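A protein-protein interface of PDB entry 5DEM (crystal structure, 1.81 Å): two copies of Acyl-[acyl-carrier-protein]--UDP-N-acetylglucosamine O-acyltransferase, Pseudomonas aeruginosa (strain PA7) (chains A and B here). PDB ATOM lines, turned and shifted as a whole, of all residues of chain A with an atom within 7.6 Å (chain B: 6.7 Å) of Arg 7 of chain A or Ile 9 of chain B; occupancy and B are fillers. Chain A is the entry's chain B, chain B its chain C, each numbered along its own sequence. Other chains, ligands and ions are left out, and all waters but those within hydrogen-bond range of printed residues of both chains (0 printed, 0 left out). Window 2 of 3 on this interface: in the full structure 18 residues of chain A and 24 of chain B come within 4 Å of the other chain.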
ATOM      1  N   ILE A   4      -9.035   9.517 -16.298  1.00  0.00           N
ATOM      2  CA  ILE A   4      -9.457  10.815 -16.772  1.00  0.00           C
ATOM      3  C   ILE A   4     -10.413  10.601 -17.931  1.00  0.00           C
ATOM      4  O   ILE A   4     -10.038  10.035 -18.972  1.00  0.00           O
ATOM      5  CB  ILE A   4      -8.251  11.652 -17.246  1.00  0.00           C
ATOM      6  CG1 ILE A   4      -7.139  11.756 -16.163  1.00  0.00           C
ATOM      7  CG2 ILE A   4      -8.750  12.976 -17.800  1.00  0.00           C
ATOM      8  CD1 ILE A   4      -7.554  12.219 -14.777  1.00  0.00           C
ATOM      9  N   ASP A   5     -11.683  10.965 -17.741  1.00  0.00           N
ATOM     10  CA  ASP A   5     -12.675  10.730 -18.765  1.00  0.00           C
ATOM     11  C   ASP A   5     -12.321  11.560 -19.999  1.00  0.00           C
ATOM     12  O   ASP A   5     -11.951  12.720 -19.868  1.00  0.00           O
ATOM     13  CB  ASP A   5     -14.051  11.097 -18.251  1.00  0.00           C
ATOM     14  CG  ASP A   5     -15.154  10.606 -19.143  1.00  0.00           C
ATOM     15  OD1 ASP A   5     -15.431  11.252 -20.173  1.00  0.00           O
ATOM     16  OD2 ASP A   5     -15.806   9.610 -18.766  1.00  0.00           O
ATOM     17  N   PRO A   6     -12.482  10.981 -21.206  1.00  0.00           N
ATOM     18  CA  PRO A   6     -12.113  11.722 -22.422  1.00  0.00           C
ATOM     19  C   PRO A   6     -13.067  12.886 -22.734  1.00  0.00           C
ATOM     20  O   PRO A   6     -12.735  13.753 -23.520  1.00  0.00           O
ATOM     21  CB  PRO A   6     -12.217  10.658 -23.532  1.00  0.00           C
ATOM     22  CG  PRO A   6     -13.169   9.651 -22.989  1.00  0.00           C
ATOM     23  CD  PRO A   6     -12.900   9.599 -21.505  1.00  0.00           C
ATOM     24  N   ARG A   7     -14.187  12.962 -22.025  1.00  0.00           N
ATOM     25  CA  ARG A   7     -15.111  14.065 -22.207  1.00  0.00           C
ATOM     26  C   ARG A   7     -14.838  15.210 -21.205  1.00  0.00           C
ATOM     27  O   ARG A   7     -15.487  16.247 -21.290  1.00  0.00           O
ATOM     28  CB  ARG A   7     -16.549  13.590 -22.057  1.00  0.00           C
ATOM     29  CG  ARG A   7     -16.981  12.667 -23.195  1.00  0.00           C
ATOM     30  CD  ARG A   7     -18.146  11.786 -22.808  1.00  0.00           C
ATOM     31  NE  ARG A   7     -17.694  10.780 -21.864  1.00  0.00           N
ATOM     32  CZ  ARG A   7     -18.295   9.614 -21.662  1.00  0.00           C
ATOM     33  NH1 ARG A   7     -19.381   9.311 -22.346  1.00  0.00           N
ATOM     34  NH2 ARG A   7     -17.831   8.785 -20.744  1.00  0.00           N
ATOM     35  N   ALA A   8     -13.868  15.023 -20.311  1.00  0.00           N
ATOM     36  CA  ALA A   8     -13.385  16.104 -19.461  1.00  0.00           C
ATOM     37  C   ALA A   8     -12.426  17.043 -20.219  1.00  0.00           C
ATOM     38  O   ALA A   8     -11.814  16.652 -21.220  1.00  0.00           O
ATOM     39  CB  ALA A   8     -12.686  15.554 -18.247  1.00  0.00           C
ATOM     40  N   ILE A   9     -12.328  18.280 -19.759  1.00  0.00           N
ATOM     41  CA  ILE A   9     -11.414  19.252 -20.340  1.00  0.00           C
ATOM     42  C   ILE A   9     -10.297  19.461 -19.332  1.00  0.00           C
ATOM     43  O   ILE A   9     -10.560  19.917 -18.210  1.00  0.00           O
ATOM     44  CB  ILE A   9     -12.111  20.592 -20.669  1.00  0.00           C
ATOM     45  CG1 ILE A   9     -13.155  20.400 -21.770  1.00  0.00           C
ATOM     46  CG2 ILE A   9     -11.091  21.651 -21.080  1.00  0.00           C
ATOM     47  CD1 ILE A   9     -13.962  21.634 -22.076  1.00  0.00           C
ATOM     48  N   ILE A  10      -9.075  19.045 -19.686  1.00  0.00           N
ATOM     49  CA  ILE A  10      -7.938  19.210 -18.807  1.00  0.00           C
ATOM     50  C   ILE A  10      -6.984  20.206 -19.442  1.00  0.00           C
ATOM     51  O   ILE A  10      -6.419  19.942 -20.519  1.00  0.00           O
ATOM     52  CB  ILE A  10      -7.167  17.892 -18.567  1.00  0.00           C
ATOM     53  CG1 ILE A  10      -8.115  16.753 -18.212  1.00  0.00           C
ATOM     54  CG2 ILE A  10      -6.090  18.086 -17.512  1.00  0.00           C
ATOM     55  CD1 ILE A  10      -8.849  16.919 -16.894  1.00  0.00           C
ATOM     56  N   VAL A  22     -11.066  11.971 -12.984  1.00  0.00           N
ATOM     57  CA  VAL A  22     -11.894  13.103 -13.400  1.00  0.00           C
ATOM     58  C   VAL A  22     -13.036  12.587 -14.218  1.00  0.00           C
ATOM     59  O   VAL A  22     -12.818  11.947 -15.269  1.00  0.00           O
ATOM     60  CB  VAL A  22     -11.083  14.168 -14.180  1.00  0.00           C
ATOM     61  CG1 VAL A  22     -11.957  15.334 -14.583  1.00  0.00           C
ATOM     62  CG2 VAL A  22      -9.894  14.655 -13.367  1.00  0.00           C
ATOM     63  N   GLY A  23     -14.264  12.899 -13.800  1.00  0.00           N
ATOM     64  CA  GLY A  23     -15.436  12.486 -14.516  1.00  0.00           C
ATOM     65  C   GLY A  23     -15.748  13.245 -15.801  1.00  0.00           C
ATOM     66  O   GLY A  23     -15.134  14.257 -16.114  1.00  0.00           O
ATOM     67  N   PRO A  24     -16.758  12.781 -16.527  1.00  0.00           N
ATOM     68  CA  PRO A  24     -17.129  13.416 -17.791  1.00  0.00           C
ATOM     69  C   PRO A  24     -17.627  14.831 -17.582  1.00  0.00           C
ATOM     70  O   PRO A  24     -18.371  15.098 -16.609  1.00  0.00           O
ATOM     71  CB  PRO A  24     -18.245  12.525 -18.327  1.00  0.00           C
ATOM     72  CG  PRO A  24     -18.754  11.785 -17.134  1.00  0.00           C
ATOM     73  CD  PRO A  24     -17.579  11.587 -16.255  1.00  0.00           C
ATOM     74  N   TRP A  25     -17.358  15.672 -18.588  1.00  0.00           N
ATOM     75  CA  TRP A  25     -17.875  17.028 -18.684  1.00  0.00           C
ATOM     76  C   TRP A  25     -17.411  17.917 -17.513  1.00  0.00           C
ATOM     77  O   TRP A  25     -18.064  18.901 -17.177  1.00  0.00           O
ATOM     78  CB  TRP A  25     -19.389  17.068 -18.825  1.00  0.00           C
ATOM     79  CG  TRP A  25     -19.952  15.998 -19.738  1.00  0.00           C
ATOM     80  CD1 TRP A  25     -19.728  15.843 -21.085  1.00  0.00           C
ATOM     81  CD2 TRP A  25     -20.834  14.938 -19.355  1.00  0.00           C
ATOM     82  NE1 TRP A  25     -20.418  14.753 -21.554  1.00  0.00           N
ATOM     83  CE2 TRP A  25     -21.103  14.179 -20.518  1.00  0.00           C
ATOM     84  CE3 TRP A  25     -21.401  14.546 -18.142  1.00  0.00           C
ATOM     85  CZ2 TRP A  25     -21.906  13.064 -20.498  1.00  0.00           C
ATOM     86  CZ3 TRP A  25     -22.202  13.435 -18.121  1.00  0.00           C
ATOM     87  CH2 TRP A  25     -22.484  12.728 -19.296  1.00  0.00           C
ATOM     88  N   SER A  26     -16.283  17.545 -16.925  1.00  0.00           N
ATOM     89  CA  SER A  26     -15.644  18.366 -15.907  1.00  0.00           C
ATOM     90  C   SER A  26     -14.480  19.136 -16.519  1.00  0.00           C
ATOM     91  O   SER A  26     -13.981  18.781 -17.610  1.00  0.00           O
ATOM     92  CB  SER A  26     -15.156  17.535 -14.780  1.00  0.00           C
ATOM     93  OG  SER A  26     -16.260  17.036 -14.067  1.00  0.00           O
ATOM     94  N   ILE A  27     -14.188  20.278 -15.907  1.00  0.00           N
ATOM     95  CA  ILE A  27     -13.206  21.205 -16.420  1.00  0.00           C
ATOM     96  C   ILE A  27     -12.163  21.356 -15.348  1.00  0.00           C
ATOM     97  O   ILE A  27     -12.481  21.780 -14.223  1.00  0.00           O
ATOM     98  CB  ILE A  27     -13.798  22.587 -16.757  1.00  0.00           C
ATOM     99  CG1 ILE A  27     -14.758  22.487 -17.930  1.00  0.00           C
ATOM    100  CG2 ILE A  27     -12.678  23.569 -17.101  1.00  0.00           C
ATOM    101  CD1 ILE A  27     -15.565  23.760 -18.193  1.00  0.00           C
ATOM    102  N   PRO A  42     -18.393  14.152 -12.257  1.00  0.00           N
ATOM    103  CA  PRO A  42     -18.813  14.725 -13.505  1.00  0.00           C
ATOM    104  C   PRO A  42     -19.320  16.141 -13.284  1.00  0.00           C
ATOM    105  O   PRO A  42     -19.754  16.450 -12.171  1.00  0.00           O
ATOM    106  CB  PRO A  42     -19.953  13.824 -13.934  1.00  0.00           C
ATOM    107  CG  PRO A  42     -20.565  13.386 -12.632  1.00  0.00           C
ATOM    108  CD  PRO A  42     -19.439  13.272 -11.680  1.00  0.00           C
ATOM    109  N   ASP B   5     -30.756  10.698 -25.632  1.00  0.00           N
ATOM    110  CA  ASP B   5     -29.740  11.477 -26.323  1.00  0.00           C
ATOM    111  C   ASP B   5     -28.473  10.666 -26.354  1.00  0.00           C
ATOM    112  O   ASP B   5     -28.066  10.102 -25.341  1.00  0.00           O
ATOM    113  CB  ASP B   5     -29.532  12.830 -25.626  1.00  0.00           C
ATOM    114  CG  ASP B   5     -28.748  13.791 -26.463  1.00  0.00           C
ATOM    115  OD1 ASP B   5     -27.511  13.675 -26.476  1.00  0.00           O
ATOM    116  OD2 ASP B   5     -29.355  14.724 -26.999  1.00  0.00           O
ATOM    117  N   PRO B   6     -27.781  10.652 -27.516  1.00  0.00           N
ATOM    118  CA  PRO B   6     -26.515   9.942 -27.577  1.00  0.00           C
ATOM    119  C   PRO B   6     -25.396  10.508 -26.689  1.00  0.00           C
ATOM    120  O   PRO B   6     -24.392   9.830 -26.471  1.00  0.00           O
ATOM    121  CB  PRO B   6     -26.120  10.049 -29.059  1.00  0.00           C
ATOM    122  CG  PRO B   6     -26.781  11.296 -29.529  1.00  0.00           C
ATOM    123  CD  PRO B   6     -28.080  11.364 -28.771  1.00  0.00           C
ATOM    124  N   ARG B   7     -25.581  11.707 -26.146  1.00  0.00           N
ATOM    125  CA  ARG B   7     -24.566  12.312 -25.267  1.00  0.00           C
ATOM    126  C   ARG B   7     -24.857  12.021 -23.804  1.00  0.00           C
ATOM    127  O   ARG B   7     -24.058  12.376 -22.931  1.00  0.00           O
ATOM    128  CB  ARG B   7     -24.482  13.817 -25.476  1.00  0.00           C
ATOM    129  CG  ARG B   7     -23.911  14.192 -26.836  1.00  0.00           C
ATOM    130  CD  ARG B   7     -24.315  15.580 -27.259  1.00  0.00           C
ATOM    131  NE  ARG B   7     -25.719  15.607 -27.586  1.00  0.00           N
ATOM    132  CZ  ARG B   7     -26.290  16.518 -28.358  1.00  0.00           C
ATOM    133  NH1 ARG B   7     -25.571  17.489 -28.884  1.00  0.00           N
ATOM    134  NH2 ARG B   7     -27.598  16.501 -28.542  1.00  0.00           N
ATOM    135  N   ALA B   8     -25.913  11.246 -23.554  1.00  0.00           N
ATOM    136  CA  ALA B   8     -26.187  10.751 -22.204  1.00  0.00           C
ATOM    137  C   ALA B   8     -25.394   9.485 -21.948  1.00  0.00           C
ATOM    138  O   ALA B   8     -25.002   8.783 -22.887  1.00  0.00           O
ATOM    139  CB  ALA B   8     -27.670  10.488 -22.031  1.00  0.00           C
ATOM    140  N   ILE B   9     -25.108   9.209 -20.689  1.00  0.00           N
ATOM    141  CA  ILE B   9     -24.448   7.982 -20.291  1.00  0.00           C
ATOM    142  C   ILE B   9     -25.466   7.068 -19.587  1.00  0.00           C
ATOM    143  O   ILE B   9     -26.070   7.456 -18.570  1.00  0.00           O
ATOM    144  CB  ILE B   9     -23.290   8.261 -19.327  1.00  0.00           C
ATOM    145  CG1 ILE B   9     -22.203   9.084 -20.035  1.00  0.00           C
ATOM    146  CG2 ILE B   9     -22.719   6.966 -18.788  1.00  0.00           C
ATOM    147  CD1 ILE B   9     -21.070   9.496 -19.116  1.00  0.00           C
ATOM    148  N   ILE B  10     -25.793   5.939 -20.224  1.00  0.00           N
ATOM    149  CA  ILE B  10     -26.762   5.000 -19.647  1.00  0.00           C
ATOM    150  C   ILE B  10     -26.020   3.738 -19.221  1.00  0.00           C
ATOM    151  O   ILE B  10     -25.453   3.044 -20.060  1.00  0.00           O
ATOM    152  CB  ILE B  10     -27.851   4.626 -20.661  1.00  0.00           C
ATOM    153  CG1 ILE B  10     -28.447   5.863 -21.355  1.00  0.00           C
ATOM    154  CG2 ILE B  10     -28.932   3.792 -19.997  1.00  0.00           C
ATOM    155  CD1 ILE B  10     -29.193   6.819 -20.446  1.00  0.00           C
ATOM    156  N   ASP B  11     -25.940   3.474 -17.924  1.00  0.00           N
ATOM    157  CA  ASP B  11     -25.270   2.263 -17.455  1.00  0.00           C
ATOM    158  C   ASP B  11     -25.970   1.008 -18.021  1.00  0.00           C
ATOM    159  O   ASP B  11     -27.197   0.991 -18.154  1.00  0.00           O
ATOM    160  CB  ASP B  11     -25.272   2.176 -15.930  1.00  0.00           C
ATOM    161  CG  ASP B  11     -24.397   1.050 -15.411  1.00  0.00           C
ATOM    162  OD1 ASP B  11     -24.913  -0.058 -15.169  1.00  0.00           O
ATOM    163  OD2 ASP B  11     -23.229   1.299 -15.085  1.00  0.00           O
ATOM    164  N   VAL B  22     -34.171  10.945 -22.210  1.00  0.00           N
ATOM    165  CA  VAL B  22     -33.016  11.355 -21.410  1.00  0.00           C
ATOM    166  C   VAL B  22     -32.218  12.376 -22.206  1.00  0.00           C
ATOM    167  O   VAL B  22     -31.836  12.112 -23.341  1.00  0.00           O
ATOM    168  CB  VAL B  22     -32.115  10.176 -21.046  1.00  0.00           C
ATOM    169  CG1 VAL B  22     -30.928  10.640 -20.227  1.00  0.00           C
ATOM    170  CG2 VAL B  22     -32.885   9.107 -20.293  1.00  0.00           C
ATOM    171  N   GLY B  23     -32.061  13.571 -21.634  1.00  0.00           N
ATOM    172  CA  GLY B  23     -31.373  14.645 -22.291  1.00  0.00           C
ATOM    173  C   GLY B  23     -29.874  14.489 -22.332  1.00  0.00           C
ATOM    174  O   GLY B  23     -29.296  13.577 -21.732  1.00  0.00           O
ATOM    175  N   TRP B  25     -25.979  14.787 -21.704  1.00  0.00           N
ATOM    176  CA  TRP B  25     -25.022  14.966 -20.624  1.00  0.00           C
ATOM    177  C   TRP B  25     -25.653  14.592 -19.276  1.00  0.00           C
ATOM    178  O   TRP B  25     -25.238  15.076 -18.233  1.00  0.00           O
ATOM    179  CB  TRP B  25     -24.443  16.387 -20.578  1.00  0.00           C
ATOM    180  CG  TRP B  25     -24.133  16.967 -21.925  1.00  0.00           C
ATOM    181  CD1 TRP B  25     -23.240  16.462 -22.867  1.00  0.00           C
ATOM    182  CD2 TRP B  25     -24.725  18.107 -22.513  1.00  0.00           C
ATOM    183  NE1 TRP B  25     -23.221  17.269 -23.963  1.00  0.00           N
ATOM    184  CE2 TRP B  25     -24.162  18.254 -23.806  1.00  0.00           C
ATOM    185  CE3 TRP B  25     -25.685  19.032 -22.088  1.00  0.00           C
ATOM    186  CZ2 TRP B  25     -24.458  19.327 -24.615  1.00  0.00           C
ATOM    187  CZ3 TRP B  25     -26.021  20.069 -22.918  1.00  0.00           C
ATOM    188  CH2 TRP B  25     -25.368  20.241 -24.156  1.00  0.00           C
ATOM    189  N   SER B  26     -26.666  13.743 -19.336  1.00  0.00           N
ATOM    190  CA  SER B  26     -27.201  13.126 -18.147  1.00  0.00           C
ATOM    191  C   SER B  26     -26.621  11.752 -17.938  1.00  0.00           C
ATOM    192  O   SER B  26     -26.149  11.096 -18.898  1.00  0.00           O
ATOM    193  CB  SER B  26     -28.703  13.095 -18.236  1.00  0.00           C
ATOM    194  OG  SER B  26     -29.209  14.419 -18.192  1.00  0.00           O
ATOM    195  N   ILE B  27     -26.558  11.347 -16.678  1.00  0.00           N
ATOM    196  CA  ILE B  27     -26.064  10.038 -16.290  1.00  0.00           C
ATOM    197  C   ILE B  27     -27.162   9.217 -15.624  1.00  0.00           C
ATOM    198  O   ILE B  27     -27.772   9.652 -14.636  1.00  0.00           O
ATOM    199  CB  ILE B  27     -24.909  10.168 -15.308  1.00  0.00           C
ATOM    200  CG1 ILE B  27     -23.745  10.888 -15.982  1.00  0.00           C
ATOM    201  CG2 ILE B  27     -24.478   8.825 -14.770  1.00  0.00           C
ATOM    202  CD1 ILE B  27     -22.673  11.347 -15.011  1.00  0.00           C
ATOM    203  N   VAL B  28     -27.406   8.032 -16.168  1.00  0.00           N
ATOM    204  CA  VAL B  28     -28.366   7.119 -15.568  1.00  0.00           C
ATOM    205  C   VAL B  28     -27.540   5.959 -15.087  1.00  0.00           C
ATOM    206  O   VAL B  28     -27.016   5.180 -15.885  1.00  0.00           O
ATOM    207  CB  VAL B  28     -29.461   6.687 -16.545  1.00  0.00           C
ATOM    208  CG1 VAL B  28     -30.438   5.732 -15.858  1.00  0.00           C
ATOM    209  CG2 VAL B  28     -30.199   7.888 -17.111  1.00  0.00           C
ATOM    210  N   GLY B  29     -27.322   5.917 -13.775  1.00  0.00           N
ATOM    211  CA  GLY B  29     -26.363   5.042 -13.161  1.00  0.00           C
ATOM    212  C   GLY B  29     -26.835   3.599 -13.064  1.00  0.00           C
ATOM    213  O   GLY B  29     -27.981   3.271 -13.404  1.00  0.00           O
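Of the 14 printed residues of chain B, 4 touch a printed residue of chain A. Printed residues of chain B that touch a printed residue of chain A: Arg 7, Ile 9, Trp 25 and Ile 27. Hydrophobic or aromatic side chains of chain B within 4 Å of the printed part of chain A: Ile 9, Trp 25 and Ile 27. Hydrophobic or aromatic side chains of chain A within 4 Å of the printed part of chain B: Pro 24, Trp 25 and Pro 42.
Arg 7 of chain A touches Ile 9 of chain B, but with the chains exchanged Ile 9 of chain A does not touch Arg 7 of chain B (13.1 Å). Trp 25 of chain A touches Arg 7 of chain B, but with the chains exchanged Arg 7 of chain A does not touch Trp 25 of chain B (6.9 Å). Trp 25 of chain A touches Ile 9 of chain B, but with the chains exchanged Ile 9 of chain A does not touch Trp 25 of chain B (10.4 Å). Trp 25 of chain A touches Ile 27 of chain B, but with the chains exchanged Ile 27 of chain A does not touch Trp 25 of chain B (11.5 Å). Of the 7 pairs that touch across the chains among the printed residues, 1 has its exchanged pair printed and touching as well.
OD1 of Asp 5 of chain A is in salt-bridge range of NE of Arg 7 of chain A (2.9 Å). O of Arg 7 of chain A lies within hydrogen-bond range of N of Trp 25 of chain A, 3.3 Å away. The backbone carbonyl oxygen (O) of Ser 26 of chain B lies within hydrogen-bond range of the backbone NH (N) of Ile 9 of chain B (2.8 Å). The backbone carbonyl oxygen (O) of Ile 9 of chain B sits at hydrogen-bond distance from the backbone NH (N) of Val 28 of chain B (2.8 Å). OD1 of Asp 5 of chain B lies within salt-bridge range of NE of Arg 7 of chain B (2.9 Å). The backbone carbonyl oxygen of Arg 7 of chain B lies within hydrogen-bond range of the backbone NH of Trp 25 of chain B, at 3.3 Å.
Among the printed residues, merely in contact across the chains: Trp 25 of chain A with Arg 7 of chain B (3.3 Å), Trp 25 of chain A with Trp 25 of chain B (3.5 Å), Trp 25 of chain A with Ile 9 of chain B (3.5 Å), Arg 7 of chain A with Ile 9 of chain B (3.6 Å), Trp 25 of chain A with Ile 27 of chain B (3.7 Å), Pro 42 of chain A with Ile 27 of chain B (3.8 Å) and Pro 24 of chain A with Ile 9 of chain B (3.8 Å).
Arg 7 of chain A touches just one residue of chain B: Ile 9 (3.6 Å). Printed residues of chain B within 4 Å of Pro 24 of chain A: Ile 9. Printed residues of chain A within 4 Å of Arg 7 of chain B: Trp 25. Ile 9 of chain B touches just these residues of chain A: Arg 7, Pro 24 and Trp 25. Of the printed residues of chain A, Ile 27 of chain B touches Trp 25 and Pro 42. The nearest residue of chain A that does not touch Ile 9 of chain B is Asp 5 of chain A (5.3 Å).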
